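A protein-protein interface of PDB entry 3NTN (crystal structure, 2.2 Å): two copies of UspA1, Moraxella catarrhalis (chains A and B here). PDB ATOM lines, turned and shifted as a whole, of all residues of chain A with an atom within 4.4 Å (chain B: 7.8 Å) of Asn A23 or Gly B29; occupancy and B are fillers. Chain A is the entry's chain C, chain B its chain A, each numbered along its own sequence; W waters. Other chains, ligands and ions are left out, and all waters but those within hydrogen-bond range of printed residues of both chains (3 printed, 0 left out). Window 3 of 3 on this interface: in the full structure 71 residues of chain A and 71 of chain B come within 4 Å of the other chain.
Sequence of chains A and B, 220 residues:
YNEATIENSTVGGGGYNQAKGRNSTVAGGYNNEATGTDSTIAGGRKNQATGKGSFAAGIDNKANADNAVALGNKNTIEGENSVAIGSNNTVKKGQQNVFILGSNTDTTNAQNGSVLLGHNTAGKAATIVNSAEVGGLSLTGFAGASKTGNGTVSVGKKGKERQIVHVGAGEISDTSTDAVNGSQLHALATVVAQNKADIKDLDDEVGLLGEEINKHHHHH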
ATOM      1  N   GLU A   7     -24.061  -9.640 -18.675  1.00  0.00           N
ATOM      2  CA  GLU A   7     -23.722 -10.731 -17.696  1.00  0.00           C
ATOM      3  C   GLU A   7     -23.052 -11.946 -18.404  1.00  0.00           C
ATOM      4  O   GLU A   7     -23.693 -12.970 -18.659  1.00  0.00           O
ATOM      5  CB  GLU A   7     -24.996 -11.173 -16.980  1.00  0.00           C
ATOM      6  CG  GLU A   7     -25.710 -10.111 -16.193  1.00  0.00           C
ATOM      7  CD  GLU A   7     -24.968  -9.747 -14.877  1.00  0.00           C
ATOM      8  OE1 GLU A   7     -24.339 -10.674 -14.272  1.00  0.00           O
ATOM      9  OE2 GLU A   7     -25.021  -8.533 -14.485  1.00  0.00           O
ATOM     10  N   ASN A   8     -21.756 -11.814 -18.710  1.00  0.00           N
ATOM     11  CA  ASN A   8     -21.013 -12.714 -19.636  1.00  0.00           C
ATOM     12  C   ASN A   8     -21.708 -12.917 -20.993  1.00  0.00           C
ATOM     13  O   ASN A   8     -21.532 -13.960 -21.659  1.00  0.00           O
ATOM     14  CB  ASN A   8     -20.607 -14.058 -18.981  1.00  0.00           C
ATOM     15  CG  ASN A   8     -19.489 -13.905 -17.956  1.00  0.00           C
ATOM     16  OD1 ASN A   8     -19.088 -12.794 -17.604  1.00  0.00           O
ATOM     17  ND2 ASN A   8     -18.982 -15.033 -17.472  1.00  0.00           N
ATOM     18  N   GLY A  21     -29.757 -12.634 -22.143  1.00  0.00           N
ATOM     19  CA  GLY A  21     -29.659 -13.728 -21.173  1.00  0.00           C
ATOM     20  C   GLY A  21     -28.254 -13.842 -20.622  1.00  0.00           C
ATOM     21  O   GLY A  21     -27.261 -13.547 -21.312  1.00  0.00           O
ATOM     22  N   ARG A  22     -28.153 -14.272 -19.378  1.00  0.00           N
ATOM     23  CA  ARG A  22     -26.862 -14.598 -18.778  1.00  0.00           C
ATOM     24  C   ARG A  22     -26.115 -15.699 -19.584  1.00  0.00           C
ATOM     25  O   ARG A  22     -26.698 -16.738 -19.888  1.00  0.00           O
ATOM     26  CB  ARG A  22     -27.098 -15.059 -17.348  1.00  0.00           C
ATOM     27  CG  ARG A  22     -25.849 -15.041 -16.466  1.00  0.00           C
ATOM     28  CD  ARG A  22     -26.189 -15.108 -14.960  1.00  0.00           C
ATOM     29  NE  ARG A  22     -27.202 -16.118 -14.579  1.00  0.00           N
ATOM     30  CZ  ARG A  22     -27.010 -17.437 -14.583  1.00  0.00           C
ATOM     31  NH1 ARG A  22     -25.834 -17.947 -14.973  1.00  0.00           N
ATOM     32  NH2 ARG A  22     -28.001 -18.244 -14.205  1.00  0.00           N
ATOM     33  N   ASN A  23     -24.830 -15.473 -19.889  1.00  0.00           N
ATOM     34  CA  ASN A  23     -24.018 -16.313 -20.805  1.00  0.00           C
ATOM     35  C   ASN A  23     -24.559 -16.429 -22.228  1.00  0.00           C
ATOM     36  O   ASN A  23     -24.168 -17.362 -22.978  1.00  0.00           O
ATOM     37  CB  ASN A  23     -23.803 -17.740 -20.271  1.00  0.00           C
ATOM     38  CG  ASN A  23     -23.400 -17.772 -18.817  1.00  0.00           C
ATOM     39  OD1 ASN A  23     -22.519 -17.013 -18.379  1.00  0.00           O
ATOM     40  ND2 ASN A  23     -24.072 -18.643 -18.038  1.00  0.00           N
ATOM     41  N   SER A  24     -25.474 -15.544 -22.623  1.00  0.00           N
ATOM     42  CA  SER A  24     -26.024 -15.676 -23.983  1.00  0.00           C
ATOM     43  C   SER A  24     -25.052 -15.084 -25.016  1.00  0.00           C
ATOM     44  O   SER A  24     -24.201 -14.285 -24.691  1.00  0.00           O
ATOM     45  CB  SER A  24     -27.408 -15.037 -24.095  1.00  0.00           C
ATOM     46  OG  SER A  24     -27.302 -13.664 -23.749  1.00  0.00           O
ATOM     47  N   THR A  25     -25.197 -15.523 -26.253  1.00  0.00           N
ATOM     48  CA  THR A  25     -24.348 -15.165 -27.331  1.00  0.00           C
ATOM     49  C   THR A  25     -25.214 -14.926 -28.577  1.00  0.00           C
ATOM     50  O   THR A  25     -26.020 -15.775 -28.973  1.00  0.00           O
ATOM     51  CB  THR A  25     -23.416 -16.330 -27.645  1.00  0.00           C
ATOM     52  OG1 THR A  25     -22.697 -16.704 -26.461  1.00  0.00           O
ATOM     53  CG2 THR A  25     -22.475 -15.965 -28.745  1.00  0.00           C
ATOM     54  N   ASP A  38     -27.576 -19.065 -21.127  1.00  0.00           N
ATOM     55  CA  ASP A  38     -26.811 -19.976 -21.999  1.00  0.00           C
ATOM     56  C   ASP A  38     -27.449 -20.120 -23.431  1.00  0.00           C
ATOM     57  O   ASP A  38     -27.280 -21.161 -24.117  1.00  0.00           O
ATOM     58  CB  ASP A  38     -26.719 -21.380 -21.345  1.00  0.00           C
ATOM     59  CG  ASP A  38     -26.156 -21.349 -19.904  1.00  0.00           C
ATOM     60  OD1 ASP A  38     -25.354 -20.468 -19.599  1.00  0.00           O
ATOM     61  OD2 ASP A  38     -26.478 -22.247 -19.073  1.00  0.00           O
ATOM     62  N   SER A  39     -28.217 -19.136 -23.884  1.00  0.00           N
ATOM     63  CA  SER A  39     -28.782 -19.261 -25.228  1.00  0.00           C
ATOM     64  C   SER A  39     -27.776 -18.812 -26.298  1.00  0.00           C
ATOM     65  O   SER A  39     -26.802 -18.070 -26.009  1.00  0.00           O
ATOM     66  CB  SER A  39     -30.095 -18.507 -25.355  1.00  0.00           C
ATOM     67  OG  SER A  39     -29.870 -17.139 -25.120  1.00  0.00           O
ATOM     68  N   VAL B  11     -11.808 -16.245 -29.342  1.00  0.00           N
ATOM     69  CA  VAL B  11     -12.861 -16.042 -28.329  1.00  0.00           C
ATOM     70  C   VAL B  11     -13.060 -14.541 -28.477  1.00  0.00           C
ATOM     71  O   VAL B  11     -12.180 -13.780 -28.073  1.00  0.00           O
ATOM     72  CB  VAL B  11     -12.312 -16.273 -26.923  1.00  0.00           C
ATOM     73  CG1 VAL B  11     -13.429 -16.100 -25.903  1.00  0.00           C
ATOM     74  CG2 VAL B  11     -11.604 -17.631 -26.818  1.00  0.00           C
ATOM     75  N   GLY B  12     -14.187 -14.033 -28.989  1.00  0.00           N
ATOM     76  CA  GLY B  12     -15.538 -14.507 -28.812  1.00  0.00           C
ATOM     77  C   GLY B  12     -16.087 -13.437 -27.845  1.00  0.00           C
ATOM     78  O   GLY B  12     -16.348 -12.279 -28.220  1.00  0.00           O
ATOM     79  N   GLY B  13     -16.153 -13.833 -26.578  1.00  0.00           N
ATOM     80  CA  GLY B  13     -16.791 -13.076 -25.511  1.00  0.00           C
ATOM     81  C   GLY B  13     -17.025 -14.111 -24.432  1.00  0.00           C
ATOM     82  O   GLY B  13     -16.535 -15.252 -24.569  1.00  0.00           O
ATOM     83  N   GLY B  14     -17.758 -13.738 -23.380  1.00  0.00           N
ATOM     84  CA  GLY B  14     -18.032 -14.646 -22.266  1.00  0.00           C
ATOM     85  C   GLY B  14     -16.861 -14.822 -21.291  1.00  0.00           C
ATOM     86  O   GLY B  14     -15.787 -14.185 -21.432  1.00  0.00           O
ATOM     87  N   GLY B  15     -17.050 -15.703 -20.309  1.00  0.00           N
ATOM     88  CA  GLY B  15     -16.016 -15.971 -19.301  1.00  0.00           C
ATOM     89  C   GLY B  15     -15.521 -17.402 -19.371  1.00  0.00           C
ATOM     90  O   GLY B  15     -16.278 -18.302 -19.739  1.00  0.00           O
ATOM     91  N   TYR B  16     -14.241 -17.575 -19.033  1.00  0.00           N
ATOM     92  CA  TYR B  16     -13.519 -18.857 -18.995  1.00  0.00           C
ATOM     93  C   TYR B  16     -13.596 -19.679 -20.269  1.00  0.00           C
ATOM     94  O   TYR B  16     -13.564 -20.921 -20.220  1.00  0.00           O
ATOM     95  CB  TYR B  16     -13.919 -19.668 -17.765  1.00  0.00           C
ATOM     96  CG  TYR B  16     -13.707 -18.871 -16.512  1.00  0.00           C
ATOM     97  CD1 TYR B  16     -12.561 -19.050 -15.731  1.00  0.00           C
ATOM     98  CD2 TYR B  16     -14.613 -17.870 -16.136  1.00  0.00           C
ATOM     99  CE1 TYR B  16     -12.355 -18.281 -14.584  1.00  0.00           C
ATOM    100  CE2 TYR B  16     -14.399 -17.096 -14.990  1.00  0.00           C
ATOM    101  CZ  TYR B  16     -13.280 -17.312 -14.219  1.00  0.00           C
ATOM    102  OH  TYR B  16     -13.099 -16.563 -13.067  1.00  0.00           O
ATOM    103  N   ASN B  17     -13.691 -18.993 -21.403  1.00  0.00           N
ATOM    104  CA  ASN B  17     -13.712 -19.659 -22.710  1.00  0.00           C
ATOM    105  C   ASN B  17     -12.304 -19.829 -23.229  1.00  0.00           C
ATOM    106  O   ASN B  17     -11.471 -18.969 -23.017  1.00  0.00           O
ATOM    107  CB  ASN B  17     -14.560 -18.865 -23.720  1.00  0.00           C
ATOM    108  CG  ASN B  17     -16.051 -18.893 -23.383  1.00  0.00           C
ATOM    109  OD1 ASN B  17     -16.608 -19.914 -23.038  1.00  0.00           O
ATOM    110  ND2 ASN B  17     -16.689 -17.766 -23.492  1.00  0.00           N
ATOM    111  N   VAL B  26     -14.389 -20.191 -30.191  1.00  0.00           N
ATOM    112  CA  VAL B  26     -15.526 -20.181 -29.267  1.00  0.00           C
ATOM    113  C   VAL B  26     -16.241 -18.824 -29.428  1.00  0.00           C
ATOM    114  O   VAL B  26     -15.686 -17.805 -29.096  1.00  0.00           O
ATOM    115  CB  VAL B  26     -15.090 -20.360 -27.803  1.00  0.00           C
ATOM    116  CG1 VAL B  26     -16.314 -20.342 -26.893  1.00  0.00           C
ATOM    117  CG2 VAL B  26     -14.309 -21.637 -27.642  1.00  0.00           C
ATOM    118  N   ALA B  27     -17.480 -18.795 -29.891  1.00  0.00           N
ATOM    119  CA  ALA B  27     -18.125 -17.484 -30.156  1.00  0.00           C
ATOM    120  C   ALA B  27     -18.555 -16.766 -28.880  1.00  0.00           C
ATOM    121  O   ALA B  27     -18.750 -15.558 -28.899  1.00  0.00           O
ATOM    122  CB  ALA B  27     -19.308 -17.630 -31.111  1.00  0.00           C
ATOM    123  N   GLY B  28     -18.702 -17.498 -27.770  1.00  0.00           N
ATOM    124  CA  GLY B  28     -19.155 -16.884 -26.523  1.00  0.00           C
ATOM    125  C   GLY B  28     -19.614 -17.984 -25.582  1.00  0.00           C
ATOM    126  O   GLY B  28     -19.231 -19.162 -25.759  1.00  0.00           O
ATOM    127  N   GLY B  29     -20.433 -17.576 -24.589  1.00  0.00           N
ATOM    128  CA  GLY B  29     -20.871 -18.401 -23.488  1.00  0.00           C
ATOM    129  C   GLY B  29     -19.892 -18.452 -22.329  1.00  0.00           C
ATOM    130  O   GLY B  29     -19.028 -17.608 -22.161  1.00  0.00           O
ATOM    131  N   TYR B  30     -20.034 -19.498 -21.525  1.00  0.00           N
ATOM    132  CA  TYR B  30     -19.267 -19.648 -20.319  1.00  0.00           C
ATOM    133  C   TYR B  30     -18.657 -21.039 -20.204  1.00  0.00           C
ATOM    134  O   TYR B  30     -19.352 -22.034 -20.395  1.00  0.00           O
ATOM    135  CB  TYR B  30     -20.201 -19.419 -19.152  1.00  0.00           C
ATOM    136  CG  TYR B  30     -19.557 -19.621 -17.813  1.00  0.00           C
ATOM    137  CD1 TYR B  30     -18.502 -18.794 -17.387  1.00  0.00           C
ATOM    138  CD2 TYR B  30     -20.005 -20.630 -16.951  1.00  0.00           C
ATOM    139  CE1 TYR B  30     -17.925 -18.970 -16.124  1.00  0.00           C
ATOM    140  CE2 TYR B  30     -19.439 -20.802 -15.683  1.00  0.00           C
ATOM    141  CZ  TYR B  30     -18.409 -19.981 -15.289  1.00  0.00           C
ATOM    142  OH  TYR B  30     -17.843 -20.184 -14.066  1.00  0.00           O
ATOM    143  N   ASN B  31     -17.374 -21.105 -19.875  1.00  0.00           N
ATOM    144  CA  ASN B  31     -16.681 -22.375 -19.676  1.00  0.00           C
ATOM    145  C   ASN B  31     -16.687 -23.300 -20.914  1.00  0.00           C
ATOM    146  O   ASN B  31     -16.857 -24.537 -20.817  1.00  0.00           O
ATOM    147  CB  ASN B  31     -17.247 -23.122 -18.473  1.00  0.00           C
ATOM    148  CG  ASN B  31     -16.214 -23.991 -17.800  1.00  0.00           C
ATOM    149  OD1 ASN B  31     -15.008 -23.746 -17.915  1.00  0.00           O
ATOM    150  ND2 ASN B  31     -16.676 -25.001 -17.060  1.00  0.00           N
ATOM    151  N   ASN B  32     -16.487 -22.696 -22.071  1.00  0.00           N
ATOM    152  CA  ASN B  32     -16.358 -23.457 -23.295  1.00  0.00           C
ATOM    153  C   ASN B  32     -14.881 -23.693 -23.705  1.00  0.00           C
ATOM    154  O   ASN B  32     -14.099 -22.777 -23.766  1.00  0.00           O
ATOM    155  CB  ASN B  32     -17.195 -22.789 -24.399  1.00  0.00           C
ATOM    156  CG  ASN B  32     -18.697 -22.783 -24.100  1.00  0.00           C
ATOM    157  OD1 ASN B  32     -19.279 -23.803 -23.730  1.00  0.00           O
ATOM    158  ND2 ASN B  32     -19.341 -21.630 -24.307  1.00  0.00           N
ATOM    159  N   ILE B  41     -17.167 -23.864 -31.057  1.00  0.00           N
ATOM    160  CA  ILE B  41     -18.275 -23.873 -30.126  1.00  0.00           C
ATOM    161  C   ILE B  41     -19.006 -22.578 -30.364  1.00  0.00           C
ATOM    162  O   ILE B  41     -18.399 -21.507 -30.294  1.00  0.00           O
ATOM    163  CB  ILE B  41     -17.838 -24.021 -28.682  1.00  0.00           C
ATOM    164  CG1 ILE B  41     -17.082 -25.351 -28.526  1.00  0.00           C
ATOM    165  CG2 ILE B  41     -19.052 -23.957 -27.765  1.00  0.00           C
ATOM    166  CD1 ILE B  41     -16.243 -25.505 -27.212  1.00  0.00           C
ATOM    167  N   ALA B  42     -20.282 -22.702 -30.744  1.00  0.00           N
ATOM    168  CA  ALA B  42     -21.087 -21.583 -31.119  1.00  0.00           C
ATOM    169  C   ALA B  42     -21.445 -20.793 -29.837  1.00  0.00           C
ATOM    170  O   ALA B  42     -21.554 -19.578 -29.885  1.00  0.00           O
ATOM    171  CB  ALA B  42     -22.364 -22.053 -31.878  1.00  0.00           C
ATOM    172  N   GLY B  43     -21.560 -21.484 -28.697  1.00  0.00           N
ATOM    173  CA  GLY B  43     -22.003 -20.826 -27.451  1.00  0.00           C
ATOM    174  C   GLY B  43     -22.654 -21.812 -26.489  1.00  0.00           C
ATOM    175  O   GLY B  43     -22.609 -23.039 -26.703  1.00  0.00           O
ATOM    176  N   GLY B  44     -23.221 -21.279 -25.416  1.00  0.00           N
ATOM    177  CA  GLY B  44     -23.760 -22.087 -24.349  1.00  0.00           C
ATOM    178  C   GLY B  44     -22.735 -22.168 -23.233  1.00  0.00           C
ATOM    179  O   GLY B  44     -21.961 -21.225 -23.016  1.00  0.00           O
ATOM    180  N   ARG B  45     -22.696 -23.314 -22.559  1.00  0.00           N
ATOM    181  CA  ARG B  45     -22.042 -23.434 -21.287  1.00  0.00           C
ATOM    182  C   ARG B  45     -21.487 -24.847 -21.146  1.00  0.00           C
ATOM    183  O   ARG B  45     -22.167 -25.816 -21.448  1.00  0.00           O
ATOM    184  CB  ARG B  45     -23.050 -23.117 -20.153  1.00  0.00           C
ATOM    185  CG  ARG B  45     -22.504 -23.321 -18.736  1.00  0.00           C
ATOM    186  CD  ARG B  45     -23.419 -22.702 -17.603  1.00  0.00           C
ATOM    187  NE  ARG B  45     -24.784 -23.263 -17.537  1.00  0.00           N
ATOM    188  CZ  ARG B  45     -25.136 -24.315 -16.788  1.00  0.00           C
ATOM    189  NH1 ARG B  45     -24.214 -24.964 -16.058  1.00  0.00           N
ATOM    190  NH2 ARG B  45     -26.421 -24.752 -16.765  1.00  0.00           N
ATOM    191  N   LYS B  46     -20.238 -24.942 -20.689  1.00  0.00           N
ATOM    192  CA  LYS B  46     -19.627 -26.205 -20.272  1.00  0.00           C
ATOM    193  C   LYS B  46     -19.446 -27.166 -21.465  1.00  0.00           C
ATOM    194  O   LYS B  46     -19.483 -28.383 -21.300  1.00  0.00           O
ATOM    195  CB  LYS B  46     -20.467 -26.860 -19.198  1.00  0.00           C
ATOM    196  CG  LYS B  46     -19.736 -27.329 -18.012  1.00  0.00           C
ATOM    197  CD  LYS B  46     -20.733 -27.467 -16.826  1.00  0.00           C
ATOM    198  CE  LYS B  46     -21.294 -28.882 -16.643  1.00  0.00           C
ATOM    199  NZ  LYS B  46     -22.756 -28.832 -16.213  1.00  0.00           N
ATOM    200  N   ASN B  47     -19.243 -26.609 -22.655  1.00  0.00           N
ATOM    201  CA  ASN B  47     -19.030 -27.423 -23.849  1.00  0.00           C
ATOM    202  C   ASN B  47     -17.560 -27.721 -24.076  1.00  0.00           C
ATOM    203  O   ASN B  47     -16.713 -26.888 -23.753  1.00  0.00           O
ATOM    204  CB  ASN B  47     -19.560 -26.706 -25.095  1.00  0.00           C
ATOM    205  CG  ASN B  47     -21.027 -26.602 -25.095  1.00  0.00           C
ATOM    206  OD1 ASN B  47     -21.693 -27.615 -25.086  1.00  0.00           O
ATOM    207  ND2 ASN B  47     -21.561 -25.369 -25.050  1.00  0.00           N
ATOM    208  N   GLY B  58     -24.734 -25.378 -26.970  1.00  0.00           N
ATOM    209  CA  GLY B  58     -25.816 -25.688 -26.004  1.00  0.00           C
ATOM    210  C   GLY B  58     -25.174 -25.901 -24.652  1.00  0.00           C
ATOM    211  O   GLY B  58     -24.225 -25.204 -24.316  1.00  0.00           O
HETATM  212  O   HOH W   1     -21.345 -14.782 -24.283  1.00  0.00           O
HETATM  213  O   HOH W   2     -24.386 -18.618 -25.260  1.00  0.00           O
HETATM  214  O   HOH W   3     -26.544 -22.497 -26.649  1.00  0.00           O
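The backbone NH (N) of Gly B15 sits close to the side-chain amide nitrogen (ND2) of Asn A8 (3.5 Å). The backbone NH (N) of Gly B29 lies within hydrogen-bond range of the side-chain hydroxyl (OG1) of Thr A25, at 3.1 Å. The guanidinium group (NE) of Arg B45 lies within salt-bridge range of the side-chain carboxylate (OD2) of Asp A38 (2.5 Å).
N of Gly B15 lies within hydrogen-bond range of O of Gly B29. The backbone NH (N) of Tyr B30 lies within hydrogen-bond range of the backbone carbonyl oxygen (O) of Gly B44 (3.0 Å). O of Tyr B30 is in hydrogen-bond range of N of Lys B46. The backbone carbonyl oxygen of Gly B58 sits at hydrogen-bond distance from the backbone NH of Arg B45. The backbone carbonyl oxygen (O) of Glu A7 sits at hydrogen-bond distance from the backbone NH (N) of Asn A23. The side-chain carboxylate of Asp A38 lies within hydrogen-bond range of the side-chain amide nitrogen of Asn A23, 2.7 Å away.
Among the printed residues, merely in contact across the chains: Asn A23 with Tyr B30 (3.4 Å), Thr A25 with Gly B28 (3.5 Å), Asn A23 with Gly B29 (3.5 Å), Asn A8 with Gly B14 (3.6 Å), Asp A38 with Gly B44 (3.6 Å), Thr A25 with Ala B27 (3.8 Å), Asn A8 with Tyr B30 (3.8 Å) and Thr A25 with Ala B42 (3.9 Å).
Printed residues of chain B within 4 Å of Asn A8: Gly B14, Gly B15 and Tyr B30. Gly A21 touches none of the printed residues of chain B. Of chain B, only Gly B29 (3.5 Å) and Tyr B30 (3.4 Å) come within 4 Å of Asn A23. Printed residues of chain B within 4 Å of Thr A25: Ala B27 (3.8 Å), Gly B28 (3.5 Å), Gly B29 (3.1 Å) and Ala B42 (3.9 Å). Printed residues of chain B within 4 Å of Asp A38: Gly B44 (3.6 Å) and Arg B45 (2.5 Å). Printed residues of chain A within 4 Å of Ala B27: Thr A25 (3.8 Å). Printed residues of chain A within 4 Å of Gly B29: Asn A23 (3.5 Å) and Thr A25 (3.1 Å). The nearest residue of chain B that does not touch Asn A23 is Arg B45 (4.1 Å). The nearest printed residue of chain A that does not touch Ala B42 is Ser A39 (6.7 Å).
Of the 9 printed residues of chain A, 4 touch a printed residue of chain B. Along chain A the printed residues that touch a printed residue of chain B span positions 8 to 38. Hydrophobic or aromatic side chains of chain B within 4 Å of the printed part of chain A: Tyr B30. Among the printed residues, 11 pairs touch across the chains. Among the printed residues, Asp or Glu carboxylates within 4 Å of a Lys or Arg side-chain nitrogen of the other chain: Asp A38 with Arg B45 (2.5 Å).
No position is printed for both chains.
Water W2 lies within hydrogen-bond range of the backbone carbonyl oxygen of Ser A39, the backbone carbonyl oxygen of Asn A23, the side-chain hydroxyl of Thr A25 and the backbone NH of Gly B44. Water W1 lies within hydrogen-bond range of O of Asn A8, O of Ser A24, N of Gly B29 and OG1 of Thr A25. Water W3 lies within hydrogen-bond range of O of Asp A38 (3.0 Å) and N of Gly B58 (3.4 Å).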
